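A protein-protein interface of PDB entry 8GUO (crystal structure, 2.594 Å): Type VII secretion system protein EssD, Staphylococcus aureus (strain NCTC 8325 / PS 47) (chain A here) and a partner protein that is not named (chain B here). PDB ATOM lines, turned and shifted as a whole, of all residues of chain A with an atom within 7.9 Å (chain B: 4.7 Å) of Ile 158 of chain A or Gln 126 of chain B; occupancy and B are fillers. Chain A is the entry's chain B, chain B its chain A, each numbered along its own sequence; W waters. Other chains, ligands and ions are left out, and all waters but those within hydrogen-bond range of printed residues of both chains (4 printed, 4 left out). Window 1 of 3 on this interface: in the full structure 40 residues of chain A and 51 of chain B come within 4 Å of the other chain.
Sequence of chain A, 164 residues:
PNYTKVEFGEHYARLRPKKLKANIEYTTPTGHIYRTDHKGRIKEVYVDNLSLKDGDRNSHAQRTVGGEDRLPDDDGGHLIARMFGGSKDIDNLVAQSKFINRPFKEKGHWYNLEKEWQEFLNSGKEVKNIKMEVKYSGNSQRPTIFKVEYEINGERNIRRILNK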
ATOM      1  N   ASN A 112       8.524 -17.582  -0.663  1.00  0.00           N
ATOM      2  CA  ASN A 112       8.448 -16.141  -0.452  1.00  0.00           C
ATOM      3  C   ASN A 112       9.214 -15.380  -1.529  1.00  0.00           C
ATOM      4  O   ASN A 112       8.782 -14.325  -1.993  1.00  0.00           O
ATOM      5  CB  ASN A 112       8.989 -15.778   0.933  1.00  0.00           C
ATOM      6  CG  ASN A 112       8.808 -14.313   1.266  1.00  0.00           C
ATOM      7  OD1 ASN A 112       9.773 -13.548   1.287  1.00  0.00           O
ATOM      8  ND2 ASN A 112       7.573 -13.914   1.539  1.00  0.00           N
ATOM      9  N   LEU A 113      10.351 -15.941  -1.927  1.00  0.00           N
ATOM     10  CA  LEU A 113      11.238 -15.324  -2.906  1.00  0.00           C
ATOM     11  C   LEU A 113      10.704 -15.461  -4.334  1.00  0.00           C
ATOM     12  O   LEU A 113      10.767 -14.511  -5.114  1.00  0.00           O
ATOM     13  CB  LEU A 113      12.638 -15.938  -2.791  1.00  0.00           C
ATOM     14  CG  LEU A 113      13.734 -15.600  -3.800  1.00  0.00           C
ATOM     15  CD1 LEU A 113      15.069 -15.443  -3.101  1.00  0.00           C
ATOM     16  CD2 LEU A 113      13.824 -16.713  -4.821  1.00  0.00           C
ATOM     17  N   GLU A 116       7.338 -13.127  -5.041  1.00  0.00           N
ATOM     18  CA  GLU A 116       7.557 -11.716  -5.346  1.00  0.00           C
ATOM     19  C   GLU A 116       8.229 -11.528  -6.705  1.00  0.00           C
ATOM     20  O   GLU A 116       7.969 -10.546  -7.403  1.00  0.00           O
ATOM     21  CB  GLU A 116       8.386 -11.040  -4.248  1.00  0.00           C
ATOM     22  CG  GLU A 116       8.470  -9.533  -4.420  1.00  0.00           C
ATOM     23  CD  GLU A 116       8.920  -8.804  -3.173  1.00  0.00           C
ATOM     24  OE1 GLU A 116       8.070  -8.144  -2.540  1.00  0.00           O
ATOM     25  OE2 GLU A 116      10.120  -8.868  -2.836  1.00  0.00           O
ATOM     26  N   TRP A 117       9.096 -12.465  -7.073  1.00  0.00           N
ATOM     27  CA  TRP A 117       9.723 -12.445  -8.390  1.00  0.00           C
ATOM     28  C   TRP A 117       8.665 -12.476  -9.486  1.00  0.00           C
ATOM     29  O   TRP A 117       8.673 -11.647 -10.394  1.00  0.00           O
ATOM     30  CB  TRP A 117      10.686 -13.625  -8.562  1.00  0.00           C
ATOM     31  CG  TRP A 117      12.036 -13.428  -7.930  1.00  0.00           C
ATOM     32  CD1 TRP A 117      12.476 -12.325  -7.258  1.00  0.00           C
ATOM     33  CD2 TRP A 117      13.129 -14.354  -7.941  1.00  0.00           C
ATOM     34  NE1 TRP A 117      13.770 -12.512  -6.838  1.00  0.00           N
ATOM     35  CE2 TRP A 117      14.195 -13.749  -7.244  1.00  0.00           C
ATOM     36  CE3 TRP A 117      13.308 -15.636  -8.465  1.00  0.00           C
ATOM     37  CZ2 TRP A 117      15.422 -14.384  -7.062  1.00  0.00           C
ATOM     38  CZ3 TRP A 117      14.525 -16.265  -8.282  1.00  0.00           C
ATOM     39  CH2 TRP A 117      15.567 -15.638  -7.587  1.00  0.00           C
ATOM     40  N   PHE A 120       6.589  -9.346  -9.835  1.00  0.00           N
ATOM     41  CA  PHE A 120       7.344  -8.295 -10.507  1.00  0.00           C
ATOM     42  C   PHE A 120       7.343  -8.511 -12.016  1.00  0.00           C
ATOM     43  O   PHE A 120       7.190  -7.564 -12.787  1.00  0.00           O
ATOM     44  CB  PHE A 120       8.781  -8.237  -9.982  1.00  0.00           C
ATOM     45  CG  PHE A 120       8.993  -7.212  -8.905  1.00  0.00           C
ATOM     46  CD1 PHE A 120       8.969  -5.860  -9.207  1.00  0.00           C
ATOM     47  CD2 PHE A 120       9.225  -7.597  -7.593  1.00  0.00           C
ATOM     48  CE1 PHE A 120       9.164  -4.911  -8.222  1.00  0.00           C
ATOM     49  CE2 PHE A 120       9.423  -6.651  -6.603  1.00  0.00           C
ATOM     50  CZ  PHE A 120       9.393  -5.304  -6.920  1.00  0.00           C
ATOM     51  N   LYS A 131      22.048 -14.742  -8.919  1.00  0.00           N
ATOM     52  CA  LYS A 131      23.156 -15.632  -8.596  1.00  0.00           C
ATOM     53  C   LYS A 131      22.996 -16.189  -7.188  1.00  0.00           C
ATOM     54  O   LYS A 131      22.277 -15.625  -6.364  1.00  0.00           O
ATOM     55  CB  LYS A 131      24.501 -14.909  -8.726  1.00  0.00           C
ATOM     56  CG  LYS A 131      24.683 -14.118 -10.005  1.00  0.00           C
ATOM     57  CD  LYS A 131      25.876 -13.186  -9.879  1.00  0.00           C
ATOM     58  CE  LYS A 131      25.945 -12.191 -11.025  1.00  0.00           C
ATOM     59  NZ  LYS A 131      27.115 -11.280 -10.872  1.00  0.00           N
ATOM     60  N   GLU A 133      25.378 -18.218  -3.921  1.00  0.00           N
ATOM     61  CA  GLU A 133      26.573 -18.836  -3.365  1.00  0.00           C
ATOM     62  C   GLU A 133      26.137 -19.858  -2.325  1.00  0.00           C
ATOM     63  O   GLU A 133      25.223 -19.605  -1.541  1.00  0.00           O
ATOM     64  CB  GLU A 133      27.510 -17.795  -2.752  1.00  0.00           C
ATOM     65  CG  GLU A 133      28.341 -17.043  -3.774  1.00  0.00           C
ATOM     66  CD  GLU A 133      29.319 -16.071  -3.146  1.00  0.00           C
ATOM     67  OE1 GLU A 133      30.516 -16.412  -3.058  1.00  0.00           O
ATOM     68  OE2 GLU A 133      28.890 -14.969  -2.746  1.00  0.00           O
ATOM     69  N   PHE A 146      22.402 -20.710   1.601  1.00  0.00           N
ATOM     70  CA  PHE A 146      22.327 -20.023   0.317  1.00  0.00           C
ATOM     71  C   PHE A 146      22.425 -18.512   0.487  1.00  0.00           C
ATOM     72  O   PHE A 146      21.666 -17.920   1.253  1.00  0.00           O
ATOM     73  CB  PHE A 146      21.019 -20.361  -0.406  1.00  0.00           C
ATOM     74  CG  PHE A 146      20.907 -21.794  -0.843  1.00  0.00           C
ATOM     75  CD1 PHE A 146      20.416 -22.760   0.020  1.00  0.00           C
ATOM     76  CD2 PHE A 146      21.279 -22.171  -2.122  1.00  0.00           C
ATOM     77  CE1 PHE A 146      20.305 -24.075  -0.385  1.00  0.00           C
ATOM     78  CE2 PHE A 146      21.173 -23.485  -2.532  1.00  0.00           C
ATOM     79  CZ  PHE A 146      20.686 -24.440  -1.662  1.00  0.00           C
ATOM     80  N   LYS A 147      23.358 -17.889  -0.224  1.00  0.00           N
ATOM     81  CA  LYS A 147      23.351 -16.439  -0.361  1.00  0.00           C
ATOM     82  C   LYS A 147      22.805 -16.107  -1.740  1.00  0.00           C
ATOM     83  O   LYS A 147      23.486 -16.292  -2.748  1.00  0.00           O
ATOM     84  CB  LYS A 147      24.747 -15.840  -0.173  1.00  0.00           C
ATOM     85  CG  LYS A 147      24.803 -14.329  -0.366  1.00  0.00           C
ATOM     86  CD  LYS A 147      25.944 -13.938  -1.282  1.00  0.00           C
ATOM     87  CE  LYS A 147      25.453 -13.799  -2.710  1.00  0.00           C
ATOM     88  NZ  LYS A 147      26.580 -13.720  -3.673  1.00  0.00           N
ATOM     89  N   VAL A 148      21.565 -15.639  -1.781  1.00  0.00           N
ATOM     90  CA  VAL A 148      20.904 -15.333  -3.040  1.00  0.00           C
ATOM     91  C   VAL A 148      21.022 -13.851  -3.353  1.00  0.00           C
ATOM     92  O   VAL A 148      20.868 -13.011  -2.467  1.00  0.00           O
ATOM     93  CB  VAL A 148      19.419 -15.734  -3.004  1.00  0.00           C
ATOM     94  CG1 VAL A 148      18.787 -15.580  -4.379  1.00  0.00           C
ATOM     95  CG2 VAL A 148      19.276 -17.160  -2.513  1.00  0.00           C
ATOM     96  N   GLU A 149      21.307 -13.532  -4.610  1.00  0.00           N
ATOM     97  CA  GLU A 149      21.384 -12.142  -5.037  1.00  0.00           C
ATOM     98  C   GLU A 149      20.647 -11.924  -6.354  1.00  0.00           C
ATOM     99  O   GLU A 149      20.554 -12.829  -7.184  1.00  0.00           O
ATOM    100  CB  GLU A 149      22.842 -11.700  -5.170  1.00  0.00           C
ATOM    101  CG  GLU A 149      23.597 -12.376  -6.298  1.00  0.00           C
ATOM    102  CD  GLU A 149      24.975 -11.788  -6.508  1.00  0.00           C
ATOM    103  OE1 GLU A 149      25.087 -10.780  -7.236  1.00  0.00           O
ATOM    104  OE2 GLU A 149      25.946 -12.333  -5.945  1.00  0.00           O
ATOM    105  N   TYR A 150      20.124 -10.715  -6.536  1.00  0.00           N
ATOM    106  CA  TYR A 150      19.383 -10.363  -7.741  1.00  0.00           C
ATOM    107  C   TYR A 150      19.199  -8.855  -7.829  1.00  0.00           C
ATOM    108  O   TYR A 150      19.276  -8.154  -6.823  1.00  0.00           O
ATOM    109  CB  TYR A 150      18.020 -11.057  -7.765  1.00  0.00           C
ATOM    110  CG  TYR A 150      17.117 -10.691  -6.608  1.00  0.00           C
ATOM    111  CD1 TYR A 150      17.242 -11.318  -5.378  1.00  0.00           C
ATOM    112  CD2 TYR A 150      16.136  -9.721  -6.750  1.00  0.00           C
ATOM    113  CE1 TYR A 150      16.417 -10.988  -4.321  1.00  0.00           C
ATOM    114  CE2 TYR A 150      15.308  -9.383  -5.700  1.00  0.00           C
ATOM    115  CZ  TYR A 150      15.452 -10.019  -4.488  1.00  0.00           C
ATOM    116  OH  TYR A 150      14.630  -9.689  -3.439  1.00  0.00           O
ATOM    117  N   GLU A 151      18.952  -8.366  -9.040  1.00  0.00           N
ATOM    118  CA  GLU A 151      18.722  -6.944  -9.272  1.00  0.00           C
ATOM    119  C   GLU A 151      17.352  -6.735  -9.911  1.00  0.00           C
ATOM    120  O   GLU A 151      16.942  -7.519 -10.767  1.00  0.00           O
ATOM    121  CB  GLU A 151      19.823  -6.361 -10.165  1.00  0.00           C
ATOM    122  CG  GLU A 151      21.240  -6.600  -9.655  1.00  0.00           C
ATOM    123  CD  GLU A 151      22.290  -5.857 -10.466  1.00  0.00           C
ATOM    124  OE1 GLU A 151      21.985  -5.445 -11.606  1.00  0.00           O
ATOM    125  OE2 GLU A 151      23.425  -5.695  -9.970  1.00  0.00           O
ATOM    126  N   GLU A 155      19.070  -2.204  -8.792  1.00  0.00           N
ATOM    127  CA  GLU A 155      19.539  -2.303  -7.419  1.00  0.00           C
ATOM    128  C   GLU A 155      19.722  -3.760  -7.013  1.00  0.00           C
ATOM    129  O   GLU A 155      18.795  -4.562  -7.112  1.00  0.00           O
ATOM    130  CB  GLU A 155      18.556  -1.612  -6.472  1.00  0.00           C
ATOM    131  CG  GLU A 155      19.210  -1.000  -5.249  1.00  0.00           C
ATOM    132  CD  GLU A 155      18.232  -0.255  -4.360  1.00  0.00           C
ATOM    133  OE1 GLU A 155      17.295  -0.892  -3.832  1.00  0.00           O
ATOM    134  OE2 GLU A 155      18.397   0.971  -4.193  1.00  0.00           O
ATOM    135  N   ARG A 156      20.922  -4.097  -6.555  1.00  0.00           N
ATOM    136  CA  ARG A 156      21.222  -5.458  -6.134  1.00  0.00           C
ATOM    137  C   ARG A 156      20.723  -5.717  -4.716  1.00  0.00           C
ATOM    138  O   ARG A 156      20.956  -4.922  -3.804  1.00  0.00           O
ATOM    139  CB  ARG A 156      22.725  -5.733  -6.222  1.00  0.00           C
ATOM    140  CG  ARG A 156      23.093  -7.211  -6.150  1.00  0.00           C
ATOM    141  CD  ARG A 156      24.551  -7.448  -6.509  1.00  0.00           C
ATOM    142  NE  ARG A 156      25.451  -7.096  -5.415  1.00  0.00           N
ATOM    143  CZ  ARG A 156      25.962  -7.970  -4.554  1.00  0.00           C
ATOM    144  NH1 ARG A 156      25.671  -9.257  -4.662  1.00  0.00           N
ATOM    145  NH2 ARG A 156      26.767  -7.555  -3.590  1.00  0.00           N
ATOM    146  N   ASN A 157      20.024  -6.832  -4.545  1.00  0.00           N
ATOM    147  CA  ASN A 157      19.563  -7.248  -3.231  1.00  0.00           C
ATOM    148  C   ASN A 157      20.187  -8.577  -2.850  1.00  0.00           C
ATOM    149  O   ASN A 157      20.437  -9.418  -3.708  1.00  0.00           O
ATOM    150  CB  ASN A 157      18.037  -7.350  -3.195  1.00  0.00           C
ATOM    151  CG  ASN A 157      17.363  -6.097  -3.709  1.00  0.00           C
ATOM    152  OD1 ASN A 157      16.873  -6.061  -4.836  1.00  0.00           O
ATOM    153  ND2 ASN A 157      17.345  -5.055  -2.885  1.00  0.00           N
ATOM    154  N   ILE A 158      20.447  -8.755  -1.562  1.00  0.00           N
ATOM    155  CA  ILE A 158      21.011 -10.003  -1.072  1.00  0.00           C
ATOM    156  C   ILE A 158      20.046 -10.644  -0.082  1.00  0.00           C
ATOM    157  O   ILE A 158      19.339  -9.948   0.647  1.00  0.00           O
ATOM    158  CB  ILE A 158      22.384  -9.780  -0.412  1.00  0.00           C
ATOM    159  CG1 ILE A 158      23.291  -8.968  -1.336  1.00  0.00           C
ATOM    160  CG2 ILE A 158      23.044 -11.104  -0.079  1.00  0.00           C
ATOM    161  CD1 ILE A 158      24.603  -8.575  -0.703  1.00  0.00           C
ATOM    162  N   ARG A 159      20.007 -11.971  -0.074  1.00  0.00           N
ATOM    163  CA  ARG A 159      19.134 -12.706   0.828  1.00  0.00           C
ATOM    164  C   ARG A 159      19.791 -14.008   1.261  1.00  0.00           C
ATOM    165  O   ARG A 159      20.539 -14.619   0.500  1.00  0.00           O
ATOM    166  CB  ARG A 159      17.785 -12.985   0.159  1.00  0.00           C
ATOM    167  CG  ARG A 159      16.741 -13.582   1.087  1.00  0.00           C
ATOM    168  CD  ARG A 159      15.415 -13.758   0.381  1.00  0.00           C
ATOM    169  NE  ARG A 159      14.360 -14.187   1.293  1.00  0.00           N
ATOM    170  CZ  ARG A 159      13.066 -13.972   1.088  1.00  0.00           C
ATOM    171  NH1 ARG A 159      12.171 -14.399   1.968  1.00  0.00           N
ATOM    172  NH2 ARG A 159      12.669 -13.324   0.004  1.00  0.00           N
ATOM    173  N   ARG A 160      19.510 -14.425   2.489  1.00  0.00           N
ATOM    174  CA  ARG A 160      20.066 -15.657   3.019  1.00  0.00           C
ATOM    175  C   ARG A 160      18.950 -16.650   3.296  1.00  0.00           C
ATOM    176  O   ARG A 160      17.944 -16.307   3.917  1.00  0.00           O
ATOM    177  CB  ARG A 160      20.873 -15.371   4.287  1.00  0.00           C
ATOM    178  CG  ARG A 160      21.844 -16.462   4.691  1.00  0.00           C
ATOM    179  CD  ARG A 160      22.961 -15.861   5.518  1.00  0.00           C
ATOM    180  NE  ARG A 160      23.544 -16.801   6.466  1.00  0.00           N
ATOM    181  CZ  ARG A 160      24.691 -16.595   7.102  1.00  0.00           C
ATOM    182  NH1 ARG A 160      25.378 -15.479   6.893  1.00  0.00           N
ATOM    183  NH2 ARG A 160      25.151 -17.501   7.952  1.00  0.00           N
ATOM    184  N   ILE A 161      19.118 -17.873   2.804  1.00  0.00           N
ATOM    185  CA  ILE A 161      18.140 -18.932   3.022  1.00  0.00           C
ATOM    186  C   ILE A 161      18.812 -20.206   3.521  1.00  0.00           C
ATOM    187  O   ILE A 161      19.811 -20.650   2.957  1.00  0.00           O
ATOM    188  CB  ILE A 161      17.350 -19.256   1.734  1.00  0.00           C
ATOM    189  CG1 ILE A 161      16.775 -17.980   1.116  1.00  0.00           C
ATOM    190  CG2 ILE A 161      16.243 -20.261   2.024  1.00  0.00           C
ATOM    191  CD1 ILE A 161      15.844 -18.229  -0.047  1.00  0.00           C
ATOM    192  N   GLU B  41      17.398 -11.168   5.715  1.00  0.00           N
ATOM    193  CA  GLU B  41      17.997 -10.104   4.918  1.00  0.00           C
ATOM    194  C   GLU B  41      18.552  -8.986   5.797  1.00  0.00           C
ATOM    195  O   GLU B  41      17.986  -8.667   6.841  1.00  0.00           O
ATOM    196  CB  GLU B  41      16.971  -9.518   3.943  1.00  0.00           C
ATOM    197  CG  GLU B  41      15.540  -9.516   4.464  1.00  0.00           C
ATOM    198  CD  GLU B  41      14.570  -8.863   3.495  1.00  0.00           C
ATOM    199  OE1 GLU B  41      14.802  -7.696   3.119  1.00  0.00           O
ATOM    200  OE2 GLU B  41      13.578  -9.516   3.109  1.00  0.00           O
ATOM    201  N   TYR B  57      23.500   0.207   0.275  1.00  0.00           N
ATOM    202  CA  TYR B  57      24.742  -0.491   0.610  1.00  0.00           C
ATOM    203  C   TYR B  57      25.373  -1.272  -0.545  1.00  0.00           C
ATOM    204  O   TYR B  57      26.594  -1.277  -0.688  1.00  0.00           O
ATOM    205  CB  TYR B  57      24.522  -1.430   1.808  1.00  0.00           C
ATOM    206  CG  TYR B  57      23.725  -2.699   1.546  1.00  0.00           C
ATOM    207  CD1 TYR B  57      24.227  -3.942   1.908  1.00  0.00           C
ATOM    208  CD2 TYR B  57      22.470  -2.649   0.963  1.00  0.00           C
ATOM    209  CE1 TYR B  57      23.509  -5.104   1.688  1.00  0.00           C
ATOM    210  CE2 TYR B  57      21.737  -3.800   0.731  1.00  0.00           C
ATOM    211  CZ  TYR B  57      22.260  -5.025   1.097  1.00  0.00           C
ATOM    212  OH  TYR B  57      21.530  -6.164   0.871  1.00  0.00           O
ATOM    213  N   THR B  58      24.561  -1.914  -1.379  1.00  0.00           N
ATOM    214  CA  THR B  58      25.107  -2.710  -2.477  1.00  0.00           C
ATOM    215  C   THR B  58      25.593  -1.849  -3.641  1.00  0.00           C
ATOM    216  O   THR B  58      26.161  -2.366  -4.602  1.00  0.00           O
ATOM    217  CB  THR B  58      24.086  -3.729  -3.011  1.00  0.00           C
ATOM    218  OG1 THR B  58      22.828  -3.083  -3.231  1.00  0.00           O
ATOM    219  CG2 THR B  58      23.902  -4.867  -2.017  1.00  0.00           C
ATOM    220  N   ASP B  72      30.566  -8.833  -0.165  1.00  0.00           N
ATOM    221  CA  ASP B  72      29.593  -9.862   0.188  1.00  0.00           C
ATOM    222  C   ASP B  72      30.075 -10.747   1.333  1.00  0.00           C
ATOM    223  O   ASP B  72      29.273 -11.214   2.140  1.00  0.00           O
ATOM    224  CB  ASP B  72      29.258 -10.723  -1.036  1.00  0.00           C
ATOM    225  CG  ASP B  72      28.328 -10.021  -2.010  1.00  0.00           C
ATOM    226  OD1 ASP B  72      28.188  -8.782  -1.920  1.00  0.00           O
ATOM    227  OD2 ASP B  72      27.730 -10.712  -2.859  1.00  0.00           O
ATOM    228  N   TRP B  75      29.429  -8.811   4.304  1.00  0.00           N
ATOM    229  CA  TRP B  75      27.990  -8.865   4.542  1.00  0.00           C
ATOM    230  C   TRP B  75      27.625 -10.152   5.266  1.00  0.00           C
ATOM    231  O   TRP B  75      26.741 -10.170   6.121  1.00  0.00           O
ATOM    232  CB  TRP B  75      27.217  -8.767   3.226  1.00  0.00           C
ATOM    233  CG  TRP B  75      25.724  -8.797   3.400  1.00  0.00           C
ATOM    234  CD1 TRP B  75      24.897  -7.727   3.574  1.00  0.00           C
ATOM    235  CD2 TRP B  75      24.887  -9.960   3.426  1.00  0.00           C
ATOM    236  NE1 TRP B  75      23.600  -8.152   3.702  1.00  0.00           N
ATOM    237  CE2 TRP B  75      23.566  -9.519   3.616  1.00  0.00           C
ATOM    238  CE3 TRP B  75      25.129 -11.332   3.307  1.00  0.00           C
ATOM    239  CZ2 TRP B  75      22.486 -10.399   3.690  1.00  0.00           C
ATOM    240  CZ3 TRP B  75      24.060 -12.205   3.381  1.00  0.00           C
ATOM    241  CH2 TRP B  75      22.754 -11.737   3.571  1.00  0.00           C
ATOM    242  N   PHE B 124       4.691 -11.671   2.483  1.00  0.00           N
ATOM    243  CA  PHE B 124       5.186 -10.477   1.812  1.00  0.00           C
ATOM    244  C   PHE B 124       6.657 -10.669   1.477  1.00  0.00           C
ATOM    245  O   PHE B 124       7.412 -11.232   2.269  1.00  0.00           O
ATOM    246  CB  PHE B 124       4.985  -9.226   2.670  1.00  0.00           C
ATOM    247  CG  PHE B 124       3.543  -8.875   2.902  1.00  0.00           C
ATOM    248  CD1 PHE B 124       2.727  -8.512   1.842  1.00  0.00           C
ATOM    249  CD2 PHE B 124       3.007  -8.885   4.180  1.00  0.00           C
ATOM    250  CE1 PHE B 124       1.401  -8.184   2.050  1.00  0.00           C
ATOM    251  CE2 PHE B 124       1.684  -8.556   4.394  1.00  0.00           C
ATOM    252  CZ  PHE B 124       0.879  -8.206   3.327  1.00  0.00           C
ATOM    253  N   GLY B 125       7.058 -10.203   0.299  1.00  0.00           N
ATOM    254  CA  GLY B 125       8.411 -10.410  -0.182  1.00  0.00           C
ATOM    255  C   GLY B 125       9.436  -9.435   0.368  1.00  0.00           C
ATOM    256  O   GLY B 125       9.112  -8.554   1.160  1.00  0.00           O
ATOM    257  N   GLN B 126      10.679  -9.597  -0.071  1.00  0.00           N
ATOM    258  CA  GLN B 126      11.798  -8.797   0.419  1.00  0.00           C
ATOM    259  C   GLN B 126      11.699  -7.322   0.017  1.00  0.00           C
ATOM    260  O   GLN B 126      11.940  -6.431   0.833  1.00  0.00           O
ATOM    261  CB  GLN B 126      13.116  -9.401  -0.082  1.00  0.00           C
ATOM    262  CG  GLN B 126      14.307  -8.459  -0.042  1.00  0.00           C
ATOM    263  CD  GLN B 126      15.627  -9.182  -0.246  1.00  0.00           C
ATOM    264  OE1 GLN B 126      15.698 -10.179  -0.964  1.00  0.00           O
ATOM    265  NE2 GLN B 126      16.680  -8.675   0.384  1.00  0.00           N
ATOM    266  N   ILE B 127      11.337  -7.075  -1.239  1.00  0.00           N
ATOM    267  CA  ILE B 127      11.241  -5.717  -1.763  1.00  0.00           C
ATOM    268  C   ILE B 127       9.998  -5.018  -1.224  1.00  0.00           C
ATOM    269  O   ILE B 127       9.987  -3.801  -1.037  1.00  0.00           O
ATOM    270  CB  ILE B 127      11.215  -5.711  -3.307  1.00  0.00           C
ATOM    271  CG1 ILE B 127      12.419  -6.479  -3.856  1.00  0.00           C
ATOM    272  CG2 ILE B 127      11.197  -4.285  -3.845  1.00  0.00           C
ATOM    273  CD1 ILE B 127      13.752  -5.921  -3.401  1.00  0.00           C
ATOM    274  N   GLY B 128       8.952  -5.795  -0.967  1.00  0.00           N
ATOM    275  CA  GLY B 128       7.746  -5.262  -0.366  1.00  0.00           C
ATOM    276  C   GLY B 128       8.027  -4.763   1.037  1.00  0.00           C
ATOM    277  O   GLY B 128       7.630  -3.659   1.403  1.00  0.00           O
ATOM    278  N   ARG B 129       8.715  -5.587   1.823  1.00  0.00           N
ATOM    279  CA  ARG B 129       9.167  -5.194   3.153  1.00  0.00           C
ATOM    280  C   ARG B 129      10.011  -3.926   3.095  1.00  0.00           C
ATOM    281  O   ARG B 129       9.805  -2.997   3.878  1.00  0.00           O
ATOM    282  CB  ARG B 129       9.977  -6.314   3.803  1.00  0.00           C
ATOM    283  CG  ARG B 129       9.168  -7.321   4.600  1.00  0.00           C
ATOM    284  CD  ARG B 129      10.088  -8.320   5.283  1.00  0.00           C
ATOM    285  NE  ARG B 129      10.760  -9.192   4.324  1.00  0.00           N
ATOM    286  CZ  ARG B 129      10.221 -10.299   3.823  1.00  0.00           C
ATOM    287  NH1 ARG B 129       9.004 -10.675   4.199  1.00  0.00           N
ATOM    288  NH2 ARG B 129      10.897 -11.035   2.952  1.00  0.00           N
ATOM    289  N   GLN B 130      10.958  -3.896   2.160  1.00  0.00           N
ATOM    290  CA  GLN B 130      11.896  -2.784   2.046  1.00  0.00           C
ATOM    291  C   GLN B 130      11.201  -1.493   1.637  1.00  0.00           C
ATOM    292  O   GLN B 130      11.573  -0.414   2.092  1.00  0.00           O
ATOM    293  CB  GLN B 130      13.008  -3.120   1.049  1.00  0.00           C
ATOM    294  CG  GLN B 130      14.183  -2.152   1.081  1.00  0.00           C
ATOM    295  CD  GLN B 130      15.272  -2.505   0.085  1.00  0.00           C
ATOM    296  OE1 GLN B 130      16.220  -3.221   0.410  1.00  0.00           O
ATOM    297  NE2 GLN B 130      15.144  -1.997  -1.136  1.00  0.00           N
HETATM  298  O   HOH W   1      22.719  -1.805  -5.927  1.00  0.00           O
HETATM  299  O   HOH W   2      27.222  -4.774  -5.784  1.00  0.00           O
HETATM  300  O   HOH W   3       5.710  -8.857  -1.259  1.00  0.00           O
HETATM  301  O   HOH W   4      19.934  -8.310   2.518  1.00  0.00           O
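The backbone carbonyl oxygen of Phe 124 of chain B is in hydrogen-bond range of the guanidinium group of Arg 129 of chain B (2.6 Å).
NH1 of Arg 159 of chain A sits at hydrogen-bond distance from OD1 of Asn 112 of chain A, at 2.6 Å.
OE2 of Glu 116 of chain A is in hydrogen-bond range of N of Ile 127 of chain B, at 2.7 Å.
OD2 of Asp 72 of chain B lies within salt-bridge range of NZ of Lys 147 of chain A.
The backbone carbonyl oxygen of Ile 158 of chain A is in hydrogen-bond range of the side-chain amide nitrogen of Gln 126 of chain B (3.0 Å).
NH2 of Arg 129 of chain B is in hydrogen-bond range of OD1 of Asn 112 of chain A (3.2 Å).
The side-chain carboxylate (OD1) of Asp 72 of chain B is in salt-bridge range of the guanidinium group (NH2) of Arg 156 of chain A, 2.5 Å away.
The side-chain hydroxyl (OG1) of Thr 58 of chain B sits at hydrogen-bond distance from the backbone carbonyl oxygen (O) of Arg 156 of chain A.
The side-chain hydroxyl (OH) of Tyr 150 of chain A sits at hydrogen-bond distance from the side-chain amide oxygen (OE1) of Gln 126 of chain B (2.7 Å).
The backbone NH (N) of Gln 126 of chain B sits at hydrogen-bond distance from the side-chain carboxylate (OE2) of Glu 116 of chain A (2.9 Å).
The side-chain carboxylate (OE1) of Glu 116 of chain A is in hydrogen-bond range of the backbone NH (N) of Gly 128 of chain B (3.0 Å).
O of Phe 124 of chain B is in hydrogen-bond range of ND2 of Asn 112 of chain A (2.8 Å).
Of the 20 printed residues of chain A, 11 touch a printed residue of chain B.
Of the 12 printed residues of chain B, 11 touch a printed residue of chain A.
Hydrophobic or aromatic side chains of chain B within 4 Å of the printed part of chain A: Tyr 57, Trp 75 and Ile 127.
Among the printed residues, 24 pairs touch across the chains.
Among the printed residues, Asp or Glu carboxylates within 4 Å of a Lys or Arg side-chain nitrogen of the other chain: Lys 147 of chain A with Asp 72 of chain B (3.3 Å) and Arg 156 of chain A with Asp 72 of chain B (2.5 Å).
Water W3 lies within hydrogen-bond range of the backbone NH of Gly 125 of chain B (2.5 Å) and the side-chain carboxylate of Glu 116 of chain A (2.8 Å).
Ile 161 of chain A touches none of the printed residues of chain B.
Printed residues of chain A within 4 Å of Asp 72 of chain B: Lys 147, Glu 149, Arg 156 and Ile 158.
Gln 126 of chain B touches four residues of chain A.
The nearest residue of chain A that does not touch Gln 126 of chain B is Asn 157 of chain A (4.1 Å).
The nearest printed residue of chain B that does not touch Glu 149 of chain A is Gln 126 of chain B (7.3 Å).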
